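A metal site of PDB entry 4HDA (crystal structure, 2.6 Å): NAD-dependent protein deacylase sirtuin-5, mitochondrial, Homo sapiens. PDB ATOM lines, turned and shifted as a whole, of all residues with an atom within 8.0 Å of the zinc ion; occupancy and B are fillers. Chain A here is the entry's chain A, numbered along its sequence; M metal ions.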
ATOM      1  N   ARG A 138      -1.406  15.540  -5.418  1.00  0.00           N
ATOM      2  CA  ARG A 138      -1.102  15.883  -6.796  1.00  0.00           C
ATOM      3  C   ARG A 138       0.140  16.760  -6.805  1.00  0.00           C
ATOM      4  O   ARG A 138       0.223  17.741  -6.057  1.00  0.00           O
ATOM      5  CB  ARG A 138      -2.267  16.574  -7.494  1.00  0.00           C
ATOM      6  CG  ARG A 138      -2.233  16.427  -9.013  1.00  0.00           C
ATOM      7  CD  ARG A 138      -3.613  16.580  -9.659  1.00  0.00           C
ATOM      8  NE  ARG A 138      -4.097  17.964  -9.705  1.00  0.00           N
ATOM      9  CZ  ARG A 138      -5.145  18.429  -9.041  1.00  0.00           C
ATOM     10  NH1 ARG A 138      -5.857  17.653  -8.250  1.00  0.00           N
ATOM     11  NH2 ARG A 138      -5.502  19.700  -9.152  1.00  0.00           N
ATOM     12  N   CYS A 139       1.115  16.369  -7.613  1.00  0.00           N
ATOM     13  CA  CYS A 139       2.253  17.221  -7.861  1.00  0.00           C
ATOM     14  C   CYS A 139       1.772  18.353  -8.745  1.00  0.00           C
ATOM     15  O   CYS A 139       1.277  18.138  -9.845  1.00  0.00           O
ATOM     16  CB  CYS A 139       3.386  16.455  -8.540  1.00  0.00           C
ATOM     17  SG  CYS A 139       4.776  17.501  -9.022  1.00  0.00           S
ATOM     18  N   THR A 140       1.911  19.563  -8.234  1.00  0.00           N
ATOM     19  CA  THR A 140       1.404  20.760  -8.883  1.00  0.00           C
ATOM     20  C   THR A 140       2.284  21.160 -10.058  1.00  0.00           C
ATOM     21  O   THR A 140       2.067  22.196 -10.689  1.00  0.00           O
ATOM     22  CB  THR A 140       1.371  21.912  -7.881  1.00  0.00           C
ATOM     23  OG1 THR A 140       2.651  22.035  -7.267  1.00  0.00           O
ATOM     24  CG2 THR A 140       0.339  21.628  -6.806  1.00  0.00           C
ATOM     25  N   SER A 141       3.279  20.322 -10.357  1.00  0.00           N
ATOM     26  CA  SER A 141       4.202  20.571 -11.446  1.00  0.00           C
ATOM     27  C   SER A 141       3.967  19.593 -12.591  1.00  0.00           C
ATOM     28  O   SER A 141       3.542  19.996 -13.684  1.00  0.00           O
ATOM     29  CB  SER A 141       5.644  20.460 -10.950  1.00  0.00           C
ATOM     30  OG  SER A 141       6.569  20.558 -12.023  1.00  0.00           O
ATOM     31  N   CYS A 142       4.234  18.310 -12.359  1.00  0.00           N
ATOM     32  CA  CYS A 142       3.945  17.277 -13.341  1.00  0.00           C
ATOM     33  C   CYS A 142       2.663  16.526 -12.966  1.00  0.00           C
ATOM     34  O   CYS A 142       2.634  15.304 -12.972  1.00  0.00           O
ATOM     35  CB  CYS A 142       5.097  16.281 -13.463  1.00  0.00           C
ATOM     36  SG  CYS A 142       5.289  15.147 -12.053  1.00  0.00           S
ATOM     37  N   GLY A 143       1.616  17.275 -12.649  1.00  0.00           N
ATOM     38  CA  GLY A 143       0.347  16.706 -12.238  1.00  0.00           C
ATOM     39  C   GLY A 143       0.295  15.185 -12.253  1.00  0.00           C
ATOM     40  O   GLY A 143      -0.451  14.581 -13.022  1.00  0.00           O
ATOM     41  N   VAL A 144       1.096  14.560 -11.392  1.00  0.00           N
ATOM     42  CA  VAL A 144       0.989  13.120 -11.154  1.00  0.00           C
ATOM     43  C   VAL A 144       0.178  12.905  -9.882  1.00  0.00           C
ATOM     44  O   VAL A 144       0.112  13.792  -9.032  1.00  0.00           O
ATOM     45  CB  VAL A 144       2.386  12.456 -11.030  1.00  0.00           C
ATOM     46  CG1 VAL A 144       2.307  11.153 -10.256  1.00  0.00           C
ATOM     47  CG2 VAL A 144       2.983  12.221 -12.423  1.00  0.00           C
ATOM     48  N   VAL A 145      -0.456  11.739  -9.759  1.00  0.00           N
ATOM     49  CA  VAL A 145      -1.367  11.471  -8.650  1.00  0.00           C
ATOM     50  C   VAL A 145      -0.962  10.217  -7.903  1.00  0.00           C
ATOM     51  O   VAL A 145      -0.471   9.258  -8.497  1.00  0.00           O
ATOM     52  CB  VAL A 145      -2.802  11.303  -9.153  1.00  0.00           C
ATOM     53  CG1 VAL A 145      -3.776  11.454  -8.001  1.00  0.00           C
ATOM     54  CG2 VAL A 145      -3.099  12.299 -10.268  1.00  0.00           C
ATOM     55  N   ARG A 179       7.013  17.332  -1.256  1.00  0.00           N
ATOM     56  CA  ARG A 179       7.653  17.392  -2.564  1.00  0.00           C
ATOM     57  C   ARG A 179       7.506  16.067  -3.308  1.00  0.00           C
ATOM     58  O   ARG A 179       7.852  15.013  -2.773  1.00  0.00           O
ATOM     59  CB  ARG A 179       9.142  17.702  -2.396  1.00  0.00           C
ATOM     60  CG  ARG A 179       9.482  18.621  -1.236  1.00  0.00           C
ATOM     61  CD  ARG A 179       8.945  20.033  -1.454  1.00  0.00           C
ATOM     62  NE  ARG A 179       8.997  20.428  -2.857  1.00  0.00           N
ATOM     63  CZ  ARG A 179       8.801  21.654  -3.296  1.00  0.00           C
ATOM     64  NH1 ARG A 179       8.540  22.641  -2.444  1.00  0.00           N
ATOM     65  NH2 ARG A 179       8.865  21.907  -4.603  1.00  0.00           N
ATOM     66  N   CYS A 180       7.021  16.136  -4.546  1.00  0.00           N
ATOM     67  CA  CYS A 180       6.950  14.978  -5.430  1.00  0.00           C
ATOM     68  C   CYS A 180       8.275  14.208  -5.506  1.00  0.00           C
ATOM     69  O   CYS A 180       9.314  14.804  -5.797  1.00  0.00           O
ATOM     70  CB  CYS A 180       6.551  15.467  -6.821  1.00  0.00           C
ATOM     71  SG  CYS A 180       6.651  14.237  -8.127  1.00  0.00           S
ATOM     72  N   GLU A 181       8.245  12.905  -5.255  1.00  0.00           N
ATOM     73  CA  GLU A 181       9.453  12.085  -5.372  1.00  0.00           C
ATOM     74  C   GLU A 181       9.757  11.708  -6.823  1.00  0.00           C
ATOM     75  O   GLU A 181      10.812  11.148  -7.111  1.00  0.00           O
ATOM     76  CB  GLU A 181       9.330  10.781  -4.573  1.00  0.00           C
ATOM     77  CG  GLU A 181       8.660  10.887  -3.234  1.00  0.00           C
ATOM     78  CD  GLU A 181       7.476   9.941  -3.114  1.00  0.00           C
ATOM     79  OE1 GLU A 181       7.137   9.280  -4.124  1.00  0.00           O
ATOM     80  OE2 GLU A 181       6.892   9.850  -2.008  1.00  0.00           O
ATOM     81  N   GLU A 182       8.836  11.993  -7.735  1.00  0.00           N
ATOM     82  CA  GLU A 182       9.062  11.702  -9.146  1.00  0.00           C
ATOM     83  C   GLU A 182      10.483  12.105  -9.506  1.00  0.00           C
ATOM     84  O   GLU A 182      10.908  13.227  -9.224  1.00  0.00           O
ATOM     85  CB  GLU A 182       8.054  12.439 -10.031  1.00  0.00           C
ATOM     86  CG  GLU A 182       6.666  11.822 -10.012  1.00  0.00           C
ATOM     87  CD  GLU A 182       6.641  10.455 -10.642  1.00  0.00           C
ATOM     88  OE1 GLU A 182       7.165  10.304 -11.768  1.00  0.00           O
ATOM     89  OE2 GLU A 182       6.115   9.508 -10.013  1.00  0.00           O
ATOM     90  N   ALA A 183      11.220  11.192 -10.124  1.00  0.00           N
ATOM     91  CA  ALA A 183      12.642  11.400 -10.358  1.00  0.00           C
ATOM     92  C   ALA A 183      12.891  12.599 -11.276  1.00  0.00           C
ATOM     93  O   ALA A 183      12.491  12.604 -12.443  1.00  0.00           O
ATOM     94  CB  ALA A 183      13.266  10.141 -10.931  1.00  0.00           C
ATOM     95  N   GLY A 184      13.565  13.608 -10.734  1.00  0.00           N
ATOM     96  CA  GLY A 184      13.861  14.829 -11.473  1.00  0.00           C
ATOM     97  C   GLY A 184      12.668  15.755 -11.643  1.00  0.00           C
ATOM     98  O   GLY A 184      12.597  16.505 -12.618  1.00  0.00           O
ATOM     99  N   CYS A 185      11.730  15.706 -10.713  1.00  0.00           N
ATOM    100  CA  CYS A 185      10.600  16.643 -10.725  1.00  0.00           C
ATOM    101  C   CYS A 185      10.623  17.494  -9.458  1.00  0.00           C
ATOM    102  O   CYS A 185      11.140  18.614  -9.463  1.00  0.00           O
ATOM    103  CB  CYS A 185       9.272  15.902 -10.836  1.00  0.00           C
ATOM    104  SG  CYS A 185       7.827  16.949 -10.518  1.00  0.00           S
ATOM    105  N   GLY A 186      10.047  16.965  -8.380  1.00  0.00           N
ATOM    106  CA  GLY A 186      10.120  17.609  -7.088  1.00  0.00           C
ATOM    107  C   GLY A 186       9.201  18.815  -6.913  1.00  0.00           C
ATOM    108  O   GLY A 186       9.333  19.560  -5.941  1.00  0.00           O
ATOM    109  N   GLY A 187       8.276  19.014  -7.848  1.00  0.00           N
ATOM    110  CA  GLY A 187       7.320  20.098  -7.741  1.00  0.00           C
ATOM    111  C   GLY A 187       6.637  20.073  -6.388  1.00  0.00           C
ATOM    112  O   GLY A 187       6.794  19.117  -5.624  1.00  0.00           O
ATOM    113  N   LEU A 188       5.879  21.121  -6.082  1.00  0.00           N
ATOM    114  CA  LEU A 188       5.201  21.219  -4.793  1.00  0.00           C
ATOM    115  C   LEU A 188       3.955  20.341  -4.767  1.00  0.00           C
ATOM    116  O   LEU A 188       3.093  20.479  -5.631  1.00  0.00           O
ATOM    117  CB  LEU A 188       4.818  22.684  -4.526  1.00  0.00           C
ATOM    118  CG  LEU A 188       3.950  22.963  -3.295  1.00  0.00           C
ATOM    119  CD1 LEU A 188       4.530  22.314  -2.048  1.00  0.00           C
ATOM    120  CD2 LEU A 188       3.778  24.469  -3.084  1.00  0.00           C
ATOM    121  N   LEU A 189       3.864  19.431  -3.809  1.00  0.00           N
ATOM    122  CA  LEU A 189       2.679  18.586  -3.725  1.00  0.00           C
ATOM    123  C   LEU A 189       1.516  19.338  -3.073  1.00  0.00           C
ATOM    124  O   LEU A 189       1.685  20.046  -2.082  1.00  0.00           O
ATOM    125  CB  LEU A 189       2.949  17.292  -2.953  1.00  0.00           C
ATOM    126  CG  LEU A 189       3.713  16.191  -3.699  1.00  0.00           C
ATOM    127  CD1 LEU A 189       3.505  14.843  -3.046  1.00  0.00           C
ATOM    128  CD2 LEU A 189       3.293  16.144  -5.153  1.00  0.00           C
HETATM  129 ZN    ZN M   1       5.968  15.770  -9.933  1.00  0.00          ZN
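N of Cys 180 lies within hydrogen-bond range of O of Gly 187 (3.2 Å).
The side-chain sulfur (SG) of Cys 180 sits close to the backbone NH (N) of Glu 182 (3.2 Å).
SG of Cys 139 sits close to N of Ser 141 (3.5 Å).
The backbone NH of Gly 186 lies close to the backbone carbonyl oxygen of Cys 180.
The backbone NH of Cys 139 is in hydrogen-bond range of the backbone carbonyl oxygen of Val 144, 3.1 Å away.
The side-chain sulfur (SG) of Cys 185 lies close to the backbone NH (N) of Gly 187 (3.4 Å).
Merely in contact with the zinc ion: Glu 182.
Of the 19 residues printed, 5 come within 4 Å of the zinc ion.
The nearest printed residue that does not touch the zinc ion is Gly 187 (4.5 Å).
The zinc ion is bound by the side-chain sulfur (SG) of Cys 185 (2.3 Å).
SG of Cys 139 is bound to the zinc ion (2.3 Å).
The zinc ion is bound by the side-chain sulfur (SG) of Cys 142, at 2.3 Å.
The zinc ion is bound by the side-chain sulfur (SG) of Cys 180 (2.5 Å).
The zinc ion has four donor atoms within binding distance.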
